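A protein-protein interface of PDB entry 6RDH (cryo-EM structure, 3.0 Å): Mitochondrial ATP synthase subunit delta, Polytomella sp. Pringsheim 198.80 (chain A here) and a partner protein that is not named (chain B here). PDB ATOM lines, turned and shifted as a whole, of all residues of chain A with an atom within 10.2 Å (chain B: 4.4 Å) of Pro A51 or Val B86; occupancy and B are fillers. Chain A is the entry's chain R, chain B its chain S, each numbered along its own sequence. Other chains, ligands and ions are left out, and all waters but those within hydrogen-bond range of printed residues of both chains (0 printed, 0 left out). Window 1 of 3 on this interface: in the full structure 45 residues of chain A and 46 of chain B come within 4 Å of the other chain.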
ATOM      1  N   GLY A  29       1.645  27.057   6.172  1.00  0.00           N
ATOM      2  CA  GLY A  29       0.817  26.591   7.253  1.00  0.00           C
ATOM      3  C   GLY A  29      -0.375  25.823   6.739  1.00  0.00           C
ATOM      4  O   GLY A  29      -0.705  25.875   5.553  1.00  0.00           O
ATOM      5  N   PRO A  30      -1.037  25.076   7.625  1.00  0.00           N
ATOM      6  CA  PRO A  30      -2.172  24.257   7.171  1.00  0.00           C
ATOM      7  C   PRO A  30      -3.395  25.070   6.787  1.00  0.00           C
ATOM      8  O   PRO A  30      -4.060  24.741   5.799  1.00  0.00           O
ATOM      9  CB  PRO A  30      -2.442  23.346   8.375  1.00  0.00           C
ATOM     10  CG  PRO A  30      -1.855  24.041   9.530  1.00  0.00           C
ATOM     11  CD  PRO A  30      -0.683  24.805   9.026  1.00  0.00           C
ATOM     12  N   PHE A  33      -2.655  26.418   3.390  1.00  0.00           N
ATOM     13  CA  PHE A  33      -2.704  25.354   2.396  1.00  0.00           C
ATOM     14  C   PHE A  33      -4.134  24.940   2.097  1.00  0.00           C
ATOM     15  O   PHE A  33      -4.439  24.557   0.967  1.00  0.00           O
ATOM     16  CB  PHE A  33      -1.895  24.152   2.884  1.00  0.00           C
ATOM     17  CG  PHE A  33      -1.700  23.069   1.851  1.00  0.00           C
ATOM     18  CD1 PHE A  33      -2.533  21.964   1.812  1.00  0.00           C
ATOM     19  CD2 PHE A  33      -0.661  23.141   0.943  1.00  0.00           C
ATOM     20  CE1 PHE A  33      -2.339  20.967   0.885  1.00  0.00           C
ATOM     21  CE2 PHE A  33      -0.470  22.147   0.015  1.00  0.00           C
ATOM     22  CZ  PHE A  33      -1.308  21.061  -0.014  1.00  0.00           C
ATOM     23  N   PRO A  48      -6.114  17.380   2.193  1.00  0.00           N
ATOM     24  CA  PRO A  48      -5.363  16.365   2.927  1.00  0.00           C
ATOM     25  C   PRO A  48      -5.136  16.781   4.363  1.00  0.00           C
ATOM     26  O   PRO A  48      -5.090  17.966   4.692  1.00  0.00           O
ATOM     27  CB  PRO A  48      -4.041  16.272   2.158  1.00  0.00           C
ATOM     28  CG  PRO A  48      -3.997  17.480   1.308  1.00  0.00           C
ATOM     29  CD  PRO A  48      -5.409  17.769   0.964  1.00  0.00           C
ATOM     30  N   GLU A  49      -5.020  15.786   5.228  1.00  0.00           N
ATOM     31  CA  GLU A  49      -4.699  16.074   6.608  1.00  0.00           C
ATOM     32  C   GLU A  49      -3.217  16.390   6.739  1.00  0.00           C
ATOM     33  O   GLU A  49      -2.420  16.178   5.825  1.00  0.00           O
ATOM     34  CB  GLU A  49      -5.087  14.901   7.495  1.00  0.00           C
ATOM     35  CG  GLU A  49      -6.530  14.522   7.339  1.00  0.00           C
ATOM     36  CD  GLU A  49      -7.471  15.439   8.079  1.00  0.00           C
ATOM     37  OE1 GLU A  49      -7.119  15.900   9.182  1.00  0.00           O
ATOM     38  OE2 GLU A  49      -8.568  15.702   7.549  1.00  0.00           O
ATOM     39  N   PHE A  50      -2.853  16.930   7.890  1.00  0.00           N
ATOM     40  CA  PHE A  50      -1.492  17.341   8.174  1.00  0.00           C
ATOM     41  C   PHE A  50      -1.112  16.814   9.544  1.00  0.00           C
ATOM     42  O   PHE A  50      -1.989  16.568  10.376  1.00  0.00           O
ATOM     43  CB  PHE A  50      -1.360  18.868   8.146  1.00  0.00           C
ATOM     44  CG  PHE A  50      -2.078  19.510   7.010  1.00  0.00           C
ATOM     45  CD1 PHE A  50      -3.317  20.092   7.198  1.00  0.00           C
ATOM     46  CD2 PHE A  50      -1.520  19.523   5.751  1.00  0.00           C
ATOM     47  CE1 PHE A  50      -3.981  20.679   6.150  1.00  0.00           C
ATOM     48  CE2 PHE A  50      -2.177  20.105   4.705  1.00  0.00           C
ATOM     49  CZ  PHE A  50      -3.408  20.684   4.903  1.00  0.00           C
ATOM     50  N   PRO A  51       0.183  16.617   9.812  1.00  0.00           N
ATOM     51  CA  PRO A  51       0.580  16.111  11.134  1.00  0.00           C
ATOM     52  C   PRO A  51       0.362  17.087  12.285  1.00  0.00           C
ATOM     53  O   PRO A  51       0.530  16.682  13.440  1.00  0.00           O
ATOM     54  CB  PRO A  51       2.069  15.784  10.956  1.00  0.00           C
ATOM     55  CG  PRO A  51       2.471  16.379   9.657  1.00  0.00           C
ATOM     56  CD  PRO A  51       1.259  16.461   8.821  1.00  0.00           C
ATOM     57  N   SER A  52      -0.014  18.341  12.025  1.00  0.00           N
ATOM     58  CA  SER A  52      -0.401  19.222  13.121  1.00  0.00           C
ATOM     59  C   SER A  52      -1.783  18.880  13.658  1.00  0.00           C
ATOM     60  O   SER A  52      -2.069  19.141  14.831  1.00  0.00           O
ATOM     61  CB  SER A  52      -0.372  20.676  12.669  1.00  0.00           C
ATOM     62  OG  SER A  52      -1.048  20.825  11.434  1.00  0.00           O
ATOM     63  N   ASN A  53      -2.650  18.302  12.827  1.00  0.00           N
ATOM     64  CA  ASN A  53      -3.998  17.978  13.274  1.00  0.00           C
ATOM     65  C   ASN A  53      -4.036  16.725  14.135  1.00  0.00           C
ATOM     66  O   ASN A  53      -5.059  16.459  14.771  1.00  0.00           O
ATOM     67  CB  ASN A  53      -4.925  17.805  12.073  1.00  0.00           C
ATOM     68  CG  ASN A  53      -4.654  18.814  10.978  1.00  0.00           C
ATOM     69  OD1 ASN A  53      -4.463  18.454   9.819  1.00  0.00           O
ATOM     70  ND2 ASN A  53      -4.637  20.089  11.342  1.00  0.00           N
ATOM     71  N   TYR A  54      -2.957  15.952  14.173  1.00  0.00           N
ATOM     72  CA  TYR A  54      -2.893  14.746  14.983  1.00  0.00           C
ATOM     73  C   TYR A  54      -2.033  14.922  16.222  1.00  0.00           C
ATOM     74  O   TYR A  54      -1.787  13.947  16.937  1.00  0.00           O
ATOM     75  CB  TYR A  54      -2.373  13.577  14.149  1.00  0.00           C
ATOM     76  CG  TYR A  54      -3.236  13.291  12.954  1.00  0.00           C
ATOM     77  CD1 TYR A  54      -4.582  13.015  13.110  1.00  0.00           C
ATOM     78  CD2 TYR A  54      -2.711  13.309  11.673  1.00  0.00           C
ATOM     79  CE1 TYR A  54      -5.379  12.761  12.030  1.00  0.00           C
ATOM     80  CE2 TYR A  54      -3.502  13.052  10.584  1.00  0.00           C
ATOM     81  CZ  TYR A  54      -4.834  12.778  10.772  1.00  0.00           C
ATOM     82  OH  TYR A  54      -5.638  12.514   9.700  1.00  0.00           O
ATOM     83  N   THR A  55      -1.570  16.133  16.493  1.00  0.00           N
ATOM     84  CA  THR A  55      -0.883  16.428  17.736  1.00  0.00           C
ATOM     85  C   THR A  55      -1.775  17.329  18.574  1.00  0.00           C
ATOM     86  O   THR A  55      -2.664  18.010  18.055  1.00  0.00           O
ATOM     87  CB  THR A  55       0.496  17.076  17.496  1.00  0.00           C
ATOM     88  OG1 THR A  55       1.264  17.030  18.703  1.00  0.00           O
ATOM     89  CG2 THR A  55       0.366  18.517  17.043  1.00  0.00           C
ATOM     90  N   ALA A  56      -1.572  17.287  19.883  1.00  0.00           N
ATOM     91  CA  ALA A  56      -2.396  18.060  20.797  1.00  0.00           C
ATOM     92  C   ALA A  56      -1.585  19.074  21.582  1.00  0.00           C
ATOM     93  O   ALA A  56      -1.944  20.255  21.613  1.00  0.00           O
ATOM     94  CB  ALA A  56      -3.138  17.121  21.755  1.00  0.00           C
ATOM     95  N   VAL A  57      -0.490  18.649  22.198  1.00  0.00           N
ATOM     96  CA  VAL A  57       0.335  19.548  22.995  1.00  0.00           C
ATOM     97  C   VAL A  57       1.231  20.317  22.034  1.00  0.00           C
ATOM     98  O   VAL A  57       2.022  19.721  21.302  1.00  0.00           O
ATOM     99  CB  VAL A  57       1.167  18.781  24.025  1.00  0.00           C
ATOM    100  CG1 VAL A  57       1.902  19.755  24.913  1.00  0.00           C
ATOM    101  CG2 VAL A  57       0.301  17.831  24.829  1.00  0.00           C
ATOM    102  N   LYS A  58       1.109  21.635  22.024  1.00  0.00           N
ATOM    103  CA  LYS A  58       1.968  22.451  21.185  1.00  0.00           C
ATOM    104  C   LYS A  58       3.173  22.910  22.003  1.00  0.00           C
ATOM    105  O   LYS A  58       3.421  22.421  23.108  1.00  0.00           O
ATOM    106  CB  LYS A  58       1.179  23.615  20.591  1.00  0.00           C
ATOM    107  CG  LYS A  58       0.679  23.356  19.183  1.00  0.00           C
ATOM    108  CD  LYS A  58      -0.454  22.345  19.182  1.00  0.00           C
ATOM    109  CE  LYS A  58      -0.923  22.024  17.782  1.00  0.00           C
ATOM    110  NZ  LYS A  58      -2.084  21.095  17.816  1.00  0.00           N
ATOM    111  N   ALA A  59       3.946  23.853  21.469  1.00  0.00           N
ATOM    112  CA  ALA A  59       5.140  24.331  22.154  1.00  0.00           C
ATOM    113  C   ALA A  59       4.979  25.738  22.712  1.00  0.00           C
ATOM    114  O   ALA A  59       5.276  25.979  23.883  1.00  0.00           O
ATOM    115  CB  ALA A  59       6.344  24.285  21.208  1.00  0.00           C
ATOM    116  N   VAL A  60       4.507  26.679  21.895  1.00  0.00           N
ATOM    117  CA  VAL A  60       4.460  28.076  22.311  1.00  0.00           C
ATOM    118  C   VAL A  60       3.287  28.357  23.248  1.00  0.00           C
ATOM    119  O   VAL A  60       3.369  29.280  24.069  1.00  0.00           O
ATOM    120  CB  VAL A  60       4.413  28.970  21.059  1.00  0.00           C
ATOM    121  CG1 VAL A  60       4.747  30.424  21.393  1.00  0.00           C
ATOM    122  CG2 VAL A  60       5.357  28.429  19.996  1.00  0.00           C
ATOM    123  N   TYR A  75      10.067   9.013  24.007  1.00  0.00           N
ATOM    124  CA  TYR A  75       9.655   8.333  22.793  1.00  0.00           C
ATOM    125  C   TYR A  75      10.760   7.424  22.286  1.00  0.00           C
ATOM    126  O   TYR A  75      11.840   7.330  22.868  1.00  0.00           O
ATOM    127  CB  TYR A  75       9.292   9.344  21.722  1.00  0.00           C
ATOM    128  CG  TYR A  75       8.010  10.055  21.966  1.00  0.00           C
ATOM    129  CD1 TYR A  75       6.902   9.379  22.427  1.00  0.00           C
ATOM    130  CD2 TYR A  75       7.908  11.414  21.743  1.00  0.00           C
ATOM    131  CE1 TYR A  75       5.718  10.035  22.648  1.00  0.00           C
ATOM    132  CE2 TYR A  75       6.737  12.078  21.961  1.00  0.00           C
ATOM    133  CZ  TYR A  75       5.642  11.386  22.412  1.00  0.00           C
ATOM    134  OH  TYR A  75       4.464  12.055  22.630  1.00  0.00           O
ATOM    135  N   PHE A 135      14.104  17.738  23.464  1.00  0.00           N
ATOM    136  CA  PHE A 135      13.643  19.110  23.370  1.00  0.00           C
ATOM    137  C   PHE A 135      12.879  19.470  24.630  1.00  0.00           C
ATOM    138  O   PHE A 135      11.932  18.777  25.004  1.00  0.00           O
ATOM    139  CB  PHE A 135      12.750  19.325  22.152  1.00  0.00           C
ATOM    140  CG  PHE A 135      13.164  18.545  20.949  1.00  0.00           C
ATOM    141  CD1 PHE A 135      14.418  18.699  20.403  1.00  0.00           C
ATOM    142  CD2 PHE A 135      12.289  17.667  20.357  1.00  0.00           C
ATOM    143  CE1 PHE A 135      14.793  17.977  19.302  1.00  0.00           C
ATOM    144  CE2 PHE A 135      12.657  16.949  19.253  1.00  0.00           C
ATOM    145  CZ  PHE A 135      13.909  17.105  18.727  1.00  0.00           C
ATOM    146  N   HIS A 137      10.554  22.416  25.652  1.00  0.00           N
ATOM    147  CA  HIS A 137       9.816  23.413  24.907  1.00  0.00           C
ATOM    148  C   HIS A 137       9.512  24.598  25.807  1.00  0.00           C
ATOM    149  O   HIS A 137       9.729  24.518  27.019  1.00  0.00           O
ATOM    150  CB  HIS A 137       8.551  22.773  24.340  1.00  0.00           C
ATOM    151  CG  HIS A 137       8.827  21.880  23.176  1.00  0.00           C
ATOM    152  ND1 HIS A 137       8.858  20.509  23.281  1.00  0.00           N
ATOM    153  CD2 HIS A 137       9.140  22.164  21.891  1.00  0.00           C
ATOM    154  CE1 HIS A 137       9.154  19.987  22.106  1.00  0.00           C
ATOM    155  NE2 HIS A 137       9.330  20.971  21.245  1.00  0.00           N
ATOM    156  N   ASP A 143      10.547  16.405  25.499  1.00  0.00           N
ATOM    157  CA  ASP A 143      10.346  15.432  24.434  1.00  0.00           C
ATOM    158  C   ASP A 143      11.659  14.719  24.162  1.00  0.00           C
ATOM    159  O   ASP A 143      12.424  15.131  23.293  1.00  0.00           O
ATOM    160  CB  ASP A 143       9.851  16.114  23.203  1.00  0.00           C
ATOM    161  CG  ASP A 143       8.447  16.605  23.345  1.00  0.00           C
ATOM    162  OD1 ASP A 143       7.520  15.908  22.892  1.00  0.00           O
ATOM    163  OD2 ASP A 143       8.261  17.683  23.932  1.00  0.00           O
ATOM    164  N   CYS A 145      13.777  11.956  22.482  1.00  0.00           N
ATOM    165  CA  CYS A 145      13.561  11.367  21.158  1.00  0.00           C
ATOM    166  C   CYS A 145      14.775  10.528  20.803  1.00  0.00           C
ATOM    167  O   CYS A 145      15.686  11.024  20.145  1.00  0.00           O
ATOM    168  CB  CYS A 145      13.361  12.449  20.116  1.00  0.00           C
ATOM    169  SG  CYS A 145      12.017  13.568  20.427  1.00  0.00           S
ATOM    170  N   VAL B  82       6.307  11.446  16.100  1.00  0.00           N
ATOM    171  CA  VAL B  82       6.012  12.462  15.101  1.00  0.00           C
ATOM    172  C   VAL B  82       5.692  13.793  15.764  1.00  0.00           C
ATOM    173  O   VAL B  82       6.040  14.854  15.237  1.00  0.00           O
ATOM    174  CB  VAL B  82       4.863  11.971  14.205  1.00  0.00           C
ATOM    175  CG1 VAL B  82       4.635  12.907  13.052  1.00  0.00           C
ATOM    176  CG2 VAL B  82       5.172  10.605  13.701  1.00  0.00           C
ATOM    177  N   ASP B  83       5.066  13.766  16.938  1.00  0.00           N
ATOM    178  CA  ASP B  83       4.616  14.969  17.637  1.00  0.00           C
ATOM    179  C   ASP B  83       5.691  15.959  18.107  1.00  0.00           C
ATOM    180  O   ASP B  83       5.441  17.169  18.007  1.00  0.00           O
ATOM    181  CB  ASP B  83       3.732  14.578  18.824  1.00  0.00           C
ATOM    182  CG  ASP B  83       2.668  13.574  18.451  1.00  0.00           C
ATOM    183  OD1 ASP B  83       2.738  12.425  18.931  1.00  0.00           O
ATOM    184  OD2 ASP B  83       1.763  13.927  17.664  1.00  0.00           O
ATOM    185  N   PRO B  84       6.863  15.547  18.629  1.00  0.00           N
ATOM    186  CA  PRO B  84       7.869  16.561  18.990  1.00  0.00           C
ATOM    187  C   PRO B  84       8.421  17.334  17.816  1.00  0.00           C
ATOM    188  O   PRO B  84       8.695  18.528  17.958  1.00  0.00           O
ATOM    189  CB  PRO B  84       8.968  15.739  19.666  1.00  0.00           C
ATOM    190  CG  PRO B  84       8.742  14.402  19.233  1.00  0.00           C
ATOM    191  CD  PRO B  84       7.293  14.251  19.177  1.00  0.00           C
ATOM    192  N   PHE B  85       8.570  16.707  16.659  1.00  0.00           N
ATOM    193  CA  PHE B  85       9.045  17.441  15.504  1.00  0.00           C
ATOM    194  C   PHE B  85       7.979  18.318  14.891  1.00  0.00           C
ATOM    195  O   PHE B  85       8.317  19.292  14.215  1.00  0.00           O
ATOM    196  CB  PHE B  85       9.556  16.486  14.446  1.00  0.00           C
ATOM    197  CG  PHE B  85      10.739  15.718  14.865  1.00  0.00           C
ATOM    198  CD1 PHE B  85      11.975  16.313  14.899  1.00  0.00           C
ATOM    199  CD2 PHE B  85      10.620  14.398  15.230  1.00  0.00           C
ATOM    200  CE1 PHE B  85      13.065  15.608  15.287  1.00  0.00           C
ATOM    201  CE2 PHE B  85      11.710  13.692  15.620  1.00  0.00           C
ATOM    202  CZ  PHE B  85      12.930  14.303  15.652  1.00  0.00           C
ATOM    203  N   VAL B  86       6.708  17.990  15.080  1.00  0.00           N
ATOM    204  CA  VAL B  86       5.668  18.829  14.516  1.00  0.00           C
ATOM    205  C   VAL B  86       5.306  19.950  15.481  1.00  0.00           C
ATOM    206  O   VAL B  86       4.664  20.927  15.075  1.00  0.00           O
ATOM    207  CB  VAL B  86       4.435  17.992  14.126  1.00  0.00           C
ATOM    208  CG1 VAL B  86       3.570  17.696  15.322  1.00  0.00           C
ATOM    209  CG2 VAL B  86       3.647  18.651  13.007  1.00  0.00           C
ATOM    210  N   ARG B  87       5.721  19.856  16.744  1.00  0.00           N
ATOM    211  CA  ARG B  87       5.590  20.994  17.637  1.00  0.00           C
ATOM    212  C   ARG B  87       6.864  21.816  17.733  1.00  0.00           C
ATOM    213  O   ARG B  87       6.808  22.965  18.178  1.00  0.00           O
ATOM    214  CB  ARG B  87       5.159  20.541  19.032  1.00  0.00           C
ATOM    215  CG  ARG B  87       6.232  19.876  19.841  1.00  0.00           C
ATOM    216  CD  ARG B  87       5.731  19.621  21.238  1.00  0.00           C
ATOM    217  NE  ARG B  87       4.511  18.828  21.234  1.00  0.00           N
ATOM    218  CZ  ARG B  87       4.438  17.578  21.668  1.00  0.00           C
ATOM    219  NH1 ARG B  87       5.510  16.976  22.145  1.00  0.00           N
ATOM    220  NH2 ARG B  87       3.290  16.930  21.629  1.00  0.00           N
ATOM    221  N   LEU B  88       7.999  21.270  17.310  1.00  0.00           N
ATOM    222  CA  LEU B  88       9.256  22.002  17.300  1.00  0.00           C
ATOM    223  C   LEU B  88       9.469  22.750  15.996  1.00  0.00           C
ATOM    224  O   LEU B  88       9.907  23.903  16.007  1.00  0.00           O
ATOM    225  CB  LEU B  88      10.417  21.036  17.537  1.00  0.00           C
ATOM    226  CG  LEU B  88      11.835  21.596  17.519  1.00  0.00           C
ATOM    227  CD1 LEU B  88      12.110  22.370  18.780  1.00  0.00           C
ATOM    228  CD2 LEU B  88      12.831  20.480  17.355  1.00  0.00           C
ATOM    229  N   GLY B  90       6.908  22.955  13.615  1.00  0.00           N
ATOM    230  CA  GLY B  90       5.642  23.354  13.047  1.00  0.00           C
ATOM    231  C   GLY B  90       5.207  22.433  11.918  1.00  0.00           C
ATOM    232  O   GLY B  90       5.679  21.307  11.769  1.00  0.00           O
ATOM    233  N   ASP B  91       4.299  22.953  11.096  1.00  0.00           N
ATOM    234  CA  ASP B  91       3.711  22.185  10.001  1.00  0.00           C
ATOM    235  C   ASP B  91       3.499  23.150   8.840  1.00  0.00           C
ATOM    236  O   ASP B  91       2.535  23.918   8.851  1.00  0.00           O
ATOM    237  CB  ASP B  91       2.401  21.553  10.433  1.00  0.00           C
ATOM    238  CG  ASP B  91       2.099  20.276   9.700  1.00  0.00           C
ATOM    239  OD1 ASP B  91       1.440  19.408  10.300  1.00  0.00           O
ATOM    240  OD2 ASP B  91       2.531  20.131   8.538  1.00  0.00           O
ATOM    241  N   THR B 206      -2.703  12.126   3.839  1.00  0.00           N
ATOM    242  CA  THR B 206      -1.984  13.076   4.666  1.00  0.00           C
ATOM    243  C   THR B 206      -0.748  13.525   3.915  1.00  0.00           C
ATOM    244  O   THR B 206      -0.079  12.716   3.271  1.00  0.00           O
ATOM    245  CB  THR B 206      -1.612  12.437   6.009  1.00  0.00           C
ATOM    246  OG1 THR B 206      -2.806  11.984   6.648  1.00  0.00           O
ATOM    247  CG2 THR B 206      -0.919  13.413   6.931  1.00  0.00           C
ATOM    248  N   VAL B 207      -0.471  14.821   3.961  1.00  0.00           N
ATOM    249  CA  VAL B 207       0.769  15.372   3.444  1.00  0.00           C
ATOM    250  C   VAL B 207       1.592  15.886   4.619  1.00  0.00           C
ATOM    251  O   VAL B 207       1.120  16.698   5.422  1.00  0.00           O
ATOM    252  CB  VAL B 207       0.510  16.439   2.367  1.00  0.00           C
ATOM    253  CG1 VAL B 207      -0.510  17.467   2.814  1.00  0.00           C
ATOM    254  CG2 VAL B 207       1.803  17.105   1.984  1.00  0.00           C
ATOM    255  N   ALA B 208       2.796  15.350   4.761  1.00  0.00           N
ATOM    256  CA  ALA B 208       3.677  15.674   5.869  1.00  0.00           C
ATOM    257  C   ALA B 208       4.935  16.290   5.292  1.00  0.00           C
ATOM    258  O   ALA B 208       5.616  15.661   4.479  1.00  0.00           O
ATOM    259  CB  ALA B 208       4.007  14.431   6.685  1.00  0.00           C
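The backbone carbonyl oxygen of Glu A49 is in hydrogen-bond range of the backbone NH of Val B207 (3.0 Å).
The backbone NH (N) of Ser A52 sits at hydrogen-bond distance from the side-chain carboxylate (OD1) of Asp B91, at 2.5 Å.
OD2 of Asp B83 sits at hydrogen-bond distance from OG1 of Thr A55, at 3.3 Å.
NE of Arg B87 is in hydrogen-bond range of O of Val A57 (2.6 Å).
The guanidinium group (NH1) of Arg B87 lies within salt-bridge range of the side-chain carboxylate (OD2) of Asp A143, 3.4 Å away.
The backbone nitrogen (N) of Pro A51 sits close to the side-chain carboxylate (OD1) of Asp B91 (3.1 Å).
The side-chain amide oxygen of Asn A53 lies within hydrogen-bond range of the backbone NH of Phe A50 (2.9 Å).
The backbone carbonyl oxygen (O) of Thr A55 is in hydrogen-bond range of the side-chain amino group (NZ) of Lys A58, 3.1 Å away.
O of Phe A135 sits at hydrogen-bond distance from N of Asp A143, at 2.8 Å.
ND1 of His A137 is in hydrogen-bond range of OD2 of Asp A143 (3.0 Å).
The backbone carbonyl oxygen (O) of Asp A143 is in hydrogen-bond range of the side-chain sulfur (SG) of Cys A145 (3.3 Å).
Of chain B, only Val B86, Asp B91, Val B207 and Ala B208 come within 4 Å of Pro A51.
Val B86 touches three residues of chain A.
Of chain A, only Tyr A75 (3.6 Å), Phe A135 (3.9 Å), Asp A143 (3.5 Å) and Cys A145 (3.6 Å) come within 4 Å of Pro B84.
Of the printed residues of chain A, Ala B208 touches Pro A51.
Printed residues of chain B within 4 Å of Phe A135: Pro B84, Phe B85 and Leu B88.
Printed residues of chain B within 4 Å of Pro A48: Val B207.
Of the printed residues of chain B, Ala A59 touches Arg B87 (3.3 Å).
Of the printed residues of chain B, Thr A55 touches Asp B83, Val B86 and Arg B87.
Of the printed residues of chain B, Phe A50 touches Asp B91 (3.6 Å) and Val B207 (3.6 Å).
Ala A56 touches none of the printed residues of chain B.
The nearest residue of chain B that does not touch Pro A51 is Thr B206 (4.2 Å).
Among the printed residues, merely in contact across the chains: Gly A29 with Asp B91, Pro A30 with Asp B91, Pro A48 with Val B207, Glu A49 with Thr B206, Phe A50 with Asp B91, Phe A50 with Val B207, Pro A51 with Val B86, Pro A51 with Val B207, Pro A51 with Ala B208, Ser A52 with Val B86, Tyr A54 with Asp B83, Thr A55 with Val B86, Thr A55 with Arg B87, Ala A59 with Arg B87, Tyr A75 with Pro B84, Phe A135 with Pro B84, Phe A135 with Phe B85, Phe A135 with Leu B88, His A137 with Arg B87, His A137 with Leu B88, Asp A143 with Pro B84 and Cys A145 with Pro B84.
Hydrophobic or aromatic side chains of chain A that line the printed part of chain B: Pro A30, Pro A48, Phe A50, Pro A51, Val A57, Ala A59, Tyr A75, Phe A135 and His A137.
Printed residues of chain B that touch a printed residue of chain A: Asp B83, Pro B84, Phe B85, Val B86, Arg B87, Leu B88, Asp B91, Thr B206, Val B207 and Ala B208.
Among the printed residues, 28 pairs touch across the chains.
Among the printed residues, Asp or Glu carboxylates within 4 Å of a Lys or Arg side-chain nitrogen of the other chain: Asp A143 with Arg B87.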
